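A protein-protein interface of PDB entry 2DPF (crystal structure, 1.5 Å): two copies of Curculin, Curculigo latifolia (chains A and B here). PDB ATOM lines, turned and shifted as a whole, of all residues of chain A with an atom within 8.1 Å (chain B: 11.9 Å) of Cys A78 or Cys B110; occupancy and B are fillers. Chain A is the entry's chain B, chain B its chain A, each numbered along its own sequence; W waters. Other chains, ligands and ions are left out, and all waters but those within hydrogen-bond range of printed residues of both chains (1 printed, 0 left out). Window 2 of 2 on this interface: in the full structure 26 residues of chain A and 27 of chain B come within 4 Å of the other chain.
No position is printed for both chains.
Of the 10 pairs that touch across the chains among the printed residues, none has its exchanged pair printed and touching as well.
Water W1 lies within hydrogen-bond range of NE1 of Trp B103 (2.9 Å) and O of Ser A76 (3.0 Å).
The backbone NH of Leu B102 lies within hydrogen-bond range of the backbone carbonyl oxygen of Ile A97 (2.8 Å).
The side-chain sulfur (SG) of Cys B110 is disulfide-bonded to the side-chain sulfur (SG) of Cys A78 (2.0 Å).
The side-chain sulfur of Cys A78 lies close to the backbone carbonyl oxygen of Leu B102, at 3.5 Å.
O of Trp B103 sits at hydrogen-bond distance from N of Ile A97.
Leu A58 touches none of the printed residues of chain B.
Gly A61 touches just one residue of chain B: Leu B102.
No residue of chain B comes within 4 Å of Asn A62.
Ala A77 touches none of the printed residues of chain B.
Cys A78 touches three residues of chain B.
Trp A79 touches just one residue of chain B: Leu B102 (3.96 Å).
Printed residues of chain B within 4 Å of Ile A97: Val B101 (3.7 Å), Leu B102 (2.8 Å) and Trp B103 (3.0 Å).
Of the printed residues of chain A, Trp B103 touches Ser A76 (3.5 Å), Cys A78 (3.7 Å) and Ile A97 (3.0 Å).
Leu B105 touches none of the printed residues of chain A.
Gly B109 touches none of the printed residues of chain A.
Of the printed residues of chain A, Cys B110 touches Cys A78 (2.0 Å).
The nearest residue of chain B that does not touch Cys A78 is Arg B111 (4.1 Å).
The nearest residue of chain A that does not touch Cys B110 is Trp A79 (4.4 Å).
Of the 15 printed residues of chain A, 6 touch a printed residue of chain B.
Hydrophobic or aromatic side chains of chain B that line the printed part of chain A: Val B101, Leu B102 and Trp B103.
The backbone carbonyl oxygen of Leu B102 is in hydrogen-bond range of the backbone NH of Arg B111, 3.0 Å away.
The side-chain amide oxygen (OD1) of Asn A62 lies within hydrogen-bond range of the backbone NH (N) of Cys A78, at 3.4 Å.
The backbone NH (N) of Ser A76 sits at hydrogen-bond distance from the backbone carbonyl oxygen (O) of Leu A63 (2.9 Å).
The side-chain amide nitrogen (ND2) of Asn B108 is in hydrogen-bond range of the backbone carbonyl oxygen (O) of Cys B110 (3.4 Å).
The side-chain hydroxyl (OG) of Ser A76 sits at hydrogen-bond distance from the side-chain amide oxygen (OD1) of Asn A62 (3.1 Å).
O of Val B101 lies within hydrogen-bond range of NH2 of Arg B111 (3.3 Å).
Among the printed residues, merely in contact across the chains: Gly A61 with Leu B102 (3.5 Å), Ser A76 with Trp B103 (3.5 Å), Cys A78 with Trp B103 (3.7 Å), Trp A79 with Leu B102 (3.96 Å), Tyr A85 with Leu B102 (3.7 Å) and Ile A97 with Val B101 (3.7 Å).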
ATOM      1  N   LEU A  57      18.095 -23.300  -6.846  1.00  0.00           N
ATOM      2  CA  LEU A  57      19.261 -23.331  -7.717  1.00  0.00           C
ATOM      3  C   LEU A  57      19.597 -24.798  -7.934  1.00  0.00           C
ATOM      4  O   LEU A  57      19.793 -25.541  -6.974  1.00  0.00           O
ATOM      5  CB  LEU A  57      20.445 -22.610  -7.063  1.00  0.00           C
ATOM      6  CG  LEU A  57      21.694 -22.461  -7.933  1.00  0.00           C
ATOM      7  CD1 LEU A  57      21.371 -21.614  -9.165  1.00  0.00           C
ATOM      8  CD2 LEU A  57      22.798 -21.790  -7.116  1.00  0.00           C
ATOM      9  N   LEU A  58      19.643 -25.213  -9.194  1.00  0.00           N
ATOM     10  CA  LEU A  58      19.924 -26.605  -9.530  1.00  0.00           C
ATOM     11  C   LEU A  58      21.406 -26.971  -9.481  1.00  0.00           C
ATOM     12  O   LEU A  58      22.272 -26.098  -9.398  1.00  0.00           O
ATOM     13  CB  LEU A  58      19.340 -26.930 -10.910  1.00  0.00           C
ATOM     14  CG  LEU A  58      17.842 -26.632 -11.059  1.00  0.00           C
ATOM     15  CD1 LEU A  58      17.352 -27.190 -12.374  1.00  0.00           C
ATOM     16  CD2 LEU A  58      17.066 -27.238  -9.899  1.00  0.00           C
ATOM     17  N   ASP A  60      23.157 -27.882 -11.768  1.00  0.00           N
ATOM     18  CA  ASP A  60      23.841 -27.423 -12.974  1.00  0.00           C
ATOM     19  C   ASP A  60      23.895 -25.899 -13.076  1.00  0.00           C
ATOM     20  O   ASP A  60      24.278 -25.349 -14.110  1.00  0.00           O
ATOM     21  CB  ASP A  60      23.212 -28.032 -14.246  1.00  0.00           C
ATOM     22  CG  ASP A  60      21.768 -27.605 -14.470  1.00  0.00           C
ATOM     23  OD1 ASP A  60      21.271 -26.718 -13.754  1.00  0.00           O
ATOM     24  OD2 ASP A  60      21.130 -28.168 -15.387  1.00  0.00           O
ATOM     25  N   GLY A  61      23.512 -25.229 -11.990  1.00  0.00           N
ATOM     26  CA  GLY A  61      23.559 -23.777 -11.945  1.00  0.00           C
ATOM     27  C   GLY A  61      22.330 -23.044 -12.433  1.00  0.00           C
ATOM     28  O   GLY A  61      22.261 -21.811 -12.341  1.00  0.00           O
ATOM     29  N   ASN A  62      21.368 -23.787 -12.967  1.00  0.00           N
ATOM     30  CA  ASN A  62      20.149 -23.163 -13.461  1.00  0.00           C
ATOM     31  C   ASN A  62      19.321 -22.677 -12.266  1.00  0.00           C
ATOM     32  O   ASN A  62      19.156 -23.390 -11.271  1.00  0.00           O
ATOM     33  CB  ASN A  62      19.369 -24.181 -14.301  1.00  0.00           C
ATOM     34  CG  ASN A  62      18.298 -23.536 -15.171  1.00  0.00           C
ATOM     35  OD1 ASN A  62      18.239 -22.317 -15.317  1.00  0.00           O
ATOM     36  ND2 ASN A  62      17.451 -24.370 -15.770  1.00  0.00           N
ATOM     37  N   LEU A  63      18.812 -21.451 -12.369  1.00  0.00           N
ATOM     38  CA  LEU A  63      18.018 -20.855 -11.305  1.00  0.00           C
ATOM     39  C   LEU A  63      16.582 -20.935 -11.769  1.00  0.00           C
ATOM     40  O   LEU A  63      16.249 -20.444 -12.836  1.00  0.00           O
ATOM     41  CB  LEU A  63      18.423 -19.394 -11.091  1.00  0.00           C
ATOM     42  CG  LEU A  63      17.675 -18.646  -9.986  1.00  0.00           C
ATOM     43  CD1 LEU A  63      17.989 -19.275  -8.642  1.00  0.00           C
ATOM     44  CD2 LEU A  63      18.070 -17.178  -9.987  1.00  0.00           C
ATOM     45  N   VAL A  64      15.732 -21.557 -10.967  1.00  0.00           N
ATOM     46  CA  VAL A  64      14.355 -21.712 -11.398  1.00  0.00           C
ATOM     47  C   VAL A  64      13.295 -21.373 -10.371  1.00  0.00           C
ATOM     48  O   VAL A  64      13.447 -21.632  -9.178  1.00  0.00           O
ATOM     49  CB  VAL A  64      14.123 -23.162 -11.872  1.00  0.00           C
ATOM     50  CG1 VAL A  64      12.686 -23.339 -12.350  1.00  0.00           C
ATOM     51  CG2 VAL A  64      15.093 -23.502 -13.004  1.00  0.00           C
ATOM     52  N   GLY A  75      13.128 -18.730 -15.141  1.00  0.00           N
ATOM     53  CA  GLY A  75      14.445 -19.214 -14.782  1.00  0.00           C
ATOM     54  C   GLY A  75      15.529 -18.452 -15.498  1.00  0.00           C
ATOM     55  O   GLY A  75      15.267 -17.670 -16.419  1.00  0.00           O
ATOM     56  N   SER A  76      16.765 -18.663 -15.061  1.00  0.00           N
ATOM     57  CA  SER A  76      17.890 -18.013 -15.701  1.00  0.00           C
ATOM     58  C   SER A  76      18.088 -18.699 -17.051  1.00  0.00           C
ATOM     59  O   SER A  76      18.695 -18.138 -17.961  1.00  0.00           O
ATOM     60  CB  SER A  76      19.141 -18.158 -14.833  1.00  0.00           C
ATOM     61  OG  SER A  76      19.386 -19.519 -14.522  1.00  0.00           O
ATOM     62  N   ALA A  77      17.546 -19.913 -17.168  1.00  0.00           N
ATOM     63  CA  ALA A  77      17.640 -20.719 -18.386  1.00  0.00           C
ATOM     64  C   ALA A  77      19.073 -20.738 -18.881  1.00  0.00           C
ATOM     65  O   ALA A  77      19.351 -20.531 -20.060  1.00  0.00           O
ATOM     66  CB  ALA A  77      16.710 -20.154 -19.465  1.00  0.00           C
ATOM     67  N   CYS A  78      19.976 -21.008 -17.947  1.00  0.00           N
ATOM     68  CA  CYS A  78      21.405 -21.038 -18.216  1.00  0.00           C
ATOM     69  C   CYS A  78      22.021 -22.086 -17.308  1.00  0.00           C
ATOM     70  O   CYS A  78      21.792 -22.080 -16.102  1.00  0.00           O
ATOM     71  CB  CYS A  78      21.990 -19.669 -17.901  1.00  0.00           C
ATOM     72  SG  CYS A  78      23.787 -19.558 -18.082  1.00  0.00           S
ATOM     73  N   TRP A  79      22.826 -22.974 -17.869  1.00  0.00           N
ATOM     74  CA  TRP A  79      23.412 -24.022 -17.051  1.00  0.00           C
ATOM     75  C   TRP A  79      24.779 -24.458 -17.530  1.00  0.00           C
ATOM     76  O   TRP A  79      25.165 -24.225 -18.674  1.00  0.00           O
ATOM     77  CB  TRP A  79      22.482 -25.235 -17.043  1.00  0.00           C
ATOM     78  CG  TRP A  79      22.082 -25.643 -18.436  1.00  0.00           C
ATOM     79  CD1 TRP A  79      22.809 -26.406 -19.308  1.00  0.00           C
ATOM     80  CD2 TRP A  79      20.902 -25.245 -19.141  1.00  0.00           C
ATOM     81  NE1 TRP A  79      22.154 -26.504 -20.512  1.00  0.00           N
ATOM     82  CE2 TRP A  79      20.980 -25.802 -20.438  1.00  0.00           C
ATOM     83  CE3 TRP A  79      19.785 -24.468 -18.803  1.00  0.00           C
ATOM     84  CZ2 TRP A  79      19.980 -25.608 -21.402  1.00  0.00           C
ATOM     85  CZ3 TRP A  79      18.788 -24.273 -19.764  1.00  0.00           C
ATOM     86  CH2 TRP A  79      18.897 -24.844 -21.048  1.00  0.00           C
ATOM     87  N   GLY A  80      25.496 -25.109 -16.629  1.00  0.00           N
ATOM     88  CA  GLY A  80      26.815 -25.612 -16.950  1.00  0.00           C
ATOM     89  C   GLY A  80      26.846 -27.076 -16.580  1.00  0.00           C
ATOM     90  O   GLY A  80      25.805 -27.734 -16.518  1.00  0.00           O
ATOM     91  N   TYR A  85      26.981 -24.891  -7.494  1.00  0.00           N
ATOM     92  CA  TYR A  85      26.992 -23.466  -7.789  1.00  0.00           C
ATOM     93  C   TYR A  85      26.505 -22.656  -6.603  1.00  0.00           C
ATOM     94  O   TYR A  85      25.936 -23.191  -5.646  1.00  0.00           O
ATOM     95  CB  TYR A  85      26.096 -23.164  -8.993  1.00  0.00           C
ATOM     96  CG  TYR A  85      26.582 -23.797 -10.272  1.00  0.00           C
ATOM     97  CD1 TYR A  85      27.197 -23.026 -11.268  1.00  0.00           C
ATOM     98  CD2 TYR A  85      26.474 -25.177 -10.476  1.00  0.00           C
ATOM     99  CE1 TYR A  85      27.695 -23.614 -12.424  1.00  0.00           C
ATOM    100  CE2 TYR A  85      26.971 -25.779 -11.635  1.00  0.00           C
ATOM    101  CZ  TYR A  85      27.583 -24.990 -12.602  1.00  0.00           C
ATOM    102  OH  TYR A  85      28.119 -25.574 -13.731  1.00  0.00           O
ATOM    103  N   ILE A  97      25.232 -15.830 -10.243  1.00  0.00           N
ATOM    104  CA  ILE A  97      25.428 -17.257 -10.020  1.00  0.00           C
ATOM    105  C   ILE A  97      26.865 -17.578 -10.396  1.00  0.00           C
ATOM    106  O   ILE A  97      27.282 -17.354 -11.527  1.00  0.00           O
ATOM    107  CB  ILE A  97      24.469 -18.111 -10.867  1.00  0.00           C
ATOM    108  CG1 ILE A  97      23.033 -17.785 -10.482  1.00  0.00           C
ATOM    109  CG2 ILE A  97      24.732 -19.590 -10.632  1.00  0.00           C
ATOM    110  CD1 ILE A  97      21.988 -18.547 -11.284  1.00  0.00           C
ATOM    111  N   PRO B 100      34.038 -19.473 -12.639  1.00  0.00           N
ATOM    112  CA  PRO B 100      33.707 -18.044 -12.708  1.00  0.00           C
ATOM    113  C   PRO B 100      32.199 -17.818 -12.799  1.00  0.00           C
ATOM    114  O   PRO B 100      31.419 -18.712 -12.487  1.00  0.00           O
ATOM    115  CB  PRO B 100      34.458 -17.584 -13.953  1.00  0.00           C
ATOM    116  CG  PRO B 100      34.348 -18.791 -14.866  1.00  0.00           C
ATOM    117  CD  PRO B 100      34.578 -19.965 -13.922  1.00  0.00           C
ATOM    118  N   VAL B 101      31.794 -16.626 -13.227  1.00  0.00           N
ATOM    119  CA  VAL B 101      30.373 -16.320 -13.325  1.00  0.00           C
ATOM    120  C   VAL B 101      29.699 -17.179 -14.387  1.00  0.00           C
ATOM    121  O   VAL B 101      30.196 -17.301 -15.511  1.00  0.00           O
ATOM    122  CB  VAL B 101      30.145 -14.830 -13.665  1.00  0.00           C
ATOM    123  CG1 VAL B 101      28.667 -14.584 -13.956  1.00  0.00           C
ATOM    124  CG2 VAL B 101      30.609 -13.954 -12.515  1.00  0.00           C
ATOM    125  N   LEU B 102      28.578 -17.789 -14.014  1.00  0.00           N
ATOM    126  CA  LEU B 102      27.812 -18.612 -14.940  1.00  0.00           C
ATOM    127  C   LEU B 102      26.712 -17.759 -15.537  1.00  0.00           C
ATOM    128  O   LEU B 102      26.486 -17.774 -16.748  1.00  0.00           O
ATOM    129  CB  LEU B 102      27.149 -19.789 -14.224  1.00  0.00           C
ATOM    130  CG  LEU B 102      26.075 -20.529 -15.048  1.00  0.00           C
ATOM    131  CD1 LEU B 102      26.748 -21.319 -16.145  1.00  0.00           C
ATOM    132  CD2 LEU B 102      25.268 -21.473 -14.168  1.00  0.00           C
ATOM    133  N   TRP B 103      26.035 -17.006 -14.679  1.00  0.00           N
ATOM    134  CA  TRP B 103      24.925 -16.182 -15.126  1.00  0.00           C
ATOM    135  C   TRP B 103      24.649 -14.954 -14.279  1.00  0.00           C
ATOM    136  O   TRP B 103      24.904 -14.924 -13.072  1.00  0.00           O
ATOM    137  CB  TRP B 103      23.646 -17.028 -15.152  1.00  0.00           C
ATOM    138  CG  TRP B 103      22.412 -16.270 -15.564  1.00  0.00           C
ATOM    139  CD1 TRP B 103      21.922 -16.132 -16.832  1.00  0.00           C
ATOM    140  CD2 TRP B 103      21.503 -15.570 -14.704  1.00  0.00           C
ATOM    141  NE1 TRP B 103      20.763 -15.395 -16.812  1.00  0.00           N
ATOM    142  CE2 TRP B 103      20.479 -15.038 -15.523  1.00  0.00           C
ATOM    143  CE3 TRP B 103      21.450 -15.343 -13.322  1.00  0.00           C
ATOM    144  CZ2 TRP B 103      19.411 -14.294 -15.002  1.00  0.00           C
ATOM    145  CZ3 TRP B 103      20.388 -14.603 -12.803  1.00  0.00           C
ATOM    146  CH2 TRP B 103      19.379 -14.089 -13.647  1.00  0.00           C
ATOM    147  N   SER B 104      24.100 -13.951 -14.954  1.00  0.00           N
ATOM    148  CA  SER B 104      23.671 -12.697 -14.372  1.00  0.00           C
ATOM    149  C   SER B 104      22.867 -12.088 -15.519  1.00  0.00           C
ATOM    150  O   SER B 104      22.901 -12.606 -16.637  1.00  0.00           O
ATOM    151  CB  SER B 104      24.860 -11.803 -14.014  1.00  0.00           C
ATOM    152  OG  SER B 104      25.570 -11.400 -15.170  1.00  0.00           O
ATOM    153  N   LEU B 105      22.158 -11.003 -15.253  1.00  0.00           N
ATOM    154  CA  LEU B 105      21.353 -10.342 -16.276  1.00  0.00           C
ATOM    155  C   LEU B 105      22.190  -9.670 -17.366  1.00  0.00           C
ATOM    156  O   LEU B 105      23.359  -9.341 -17.147  1.00  0.00           O
ATOM    157  CB  LEU B 105      20.444  -9.317 -15.607  1.00  0.00           C
ATOM    158  CG  LEU B 105      19.521  -9.966 -14.570  1.00  0.00           C
ATOM    159  CD1 LEU B 105      18.668  -8.915 -13.890  1.00  0.00           C
ATOM    160  CD2 LEU B 105      18.636 -10.988 -15.263  1.00  0.00           C
ATOM    161  N   GLY B 106      21.589  -9.470 -18.539  1.00  0.00           N
ATOM    162  CA  GLY B 106      22.305  -8.833 -19.634  1.00  0.00           C
ATOM    163  C   GLY B 106      22.410  -9.691 -20.884  1.00  0.00           C
ATOM    164  O   GLY B 106      22.319 -10.917 -20.800  1.00  0.00           O
ATOM    165  N   PRO B 107      22.623  -9.075 -22.060  1.00  0.00           N
ATOM    166  CA  PRO B 107      22.741  -9.775 -23.347  1.00  0.00           C
ATOM    167  C   PRO B 107      23.402 -11.145 -23.243  1.00  0.00           C
ATOM    168  O   PRO B 107      22.745 -12.145 -22.943  1.00  0.00           O
ATOM    169  CB  PRO B 107      23.556  -8.799 -24.192  1.00  0.00           C
ATOM    170  CG  PRO B 107      23.069  -7.476 -23.708  1.00  0.00           C
ATOM    171  CD  PRO B 107      23.010  -7.657 -22.202  1.00  0.00           C
ATOM    172  N   ASN B 108      24.706 -11.185 -23.496  1.00  0.00           N
ATOM    173  CA  ASN B 108      25.469 -12.426 -23.425  1.00  0.00           C
ATOM    174  C   ASN B 108      25.803 -12.708 -21.964  1.00  0.00           C
ATOM    175  O   ASN B 108      26.972 -12.851 -21.597  1.00  0.00           O
ATOM    176  CB  ASN B 108      26.762 -12.294 -24.235  1.00  0.00           C
ATOM    177  CG  ASN B 108      27.556 -13.587 -24.281  1.00  0.00           C
ATOM    178  OD1 ASN B 108      28.639 -13.642 -24.866  1.00  0.00           O
ATOM    179  ND2 ASN B 108      27.019 -14.636 -23.666  1.00  0.00           N
ATOM    180  N   GLY B 109      24.767 -12.789 -21.136  1.00  0.00           N
ATOM    181  CA  GLY B 109      24.968 -13.030 -19.719  1.00  0.00           C
ATOM    182  C   GLY B 109      25.128 -14.477 -19.296  1.00  0.00           C
ATOM    183  O   GLY B 109      25.344 -14.750 -18.115  1.00  0.00           O
ATOM    184  N   CYS B 110      25.019 -15.408 -20.238  1.00  0.00           N
ATOM    185  CA  CYS B 110      25.162 -16.820 -19.905  1.00  0.00           C
ATOM    186  C   CYS B 110      26.446 -17.404 -20.494  1.00  0.00           C
ATOM    187  O   CYS B 110      26.672 -17.350 -21.703  1.00  0.00           O
ATOM    188  CB  CYS B 110      23.944 -17.603 -20.400  1.00  0.00           C
ATOM    189  SG  CYS B 110      24.030 -19.398 -20.094  1.00  0.00           S
ATOM    190  N   ARG B 111      27.280 -17.965 -19.626  1.00  0.00           N
ATOM    191  CA  ARG B 111      28.554 -18.546 -20.036  1.00  0.00           C
ATOM    192  C   ARG B 111      28.400 -19.838 -20.835  1.00  0.00           C
ATOM    193  O   ARG B 111      27.698 -20.763 -20.420  1.00  0.00           O
ATOM    194  CB  ARG B 111      29.415 -18.809 -18.800  1.00  0.00           C
ATOM    195  CG  ARG B 111      30.825 -19.284 -19.090  1.00  0.00           C
ATOM    196  CD  ARG B 111      31.530 -19.616 -17.782  1.00  0.00           C
ATOM    197  NE  ARG B 111      30.981 -20.822 -17.167  1.00  0.00           N
ATOM    198  CZ  ARG B 111      31.029 -21.091 -15.866  1.00  0.00           C
ATOM    199  NH1 ARG B 111      30.510 -22.219 -15.401  1.00  0.00           N
ATOM    200  NH2 ARG B 111      31.574 -20.223 -15.026  1.00  0.00           N
ATOM    201  N   ARG B 112      29.084 -19.892 -21.976  1.00  0.00           N
ATOM    202  CA  ARG B 112      29.055 -21.046 -22.871  1.00  0.00           C
ATOM    203  C   ARG B 112      27.641 -21.263 -23.404  1.00  0.00           C
ATOM    204  O   ARG B 112      27.256 -22.438 -23.583  1.00  0.00           O
ATOM    205  CB  ARG B 112      29.514 -22.311 -22.136  1.00  0.00           C
ATOM    206  CG  ARG B 112      30.695 -22.115 -21.196  1.00  0.00           C
ATOM    207  CD  ARG B 112      31.942 -21.632 -21.916  1.00  0.00           C
ATOM    208  NE  ARG B 112      33.066 -21.496 -20.992  1.00  0.00           N
ATOM    209  CZ  ARG B 112      34.280 -21.079 -21.342  1.00  0.00           C
ATOM    210  NH1 ARG B 112      34.536 -20.753 -22.600  1.00  0.00           N
ATOM    211  NH2 ARG B 112      35.240 -20.990 -20.431  1.00  0.00           N
HETATM  212  O   HOH W   1      18.633 -15.210 -18.739  1.00  0.00           O
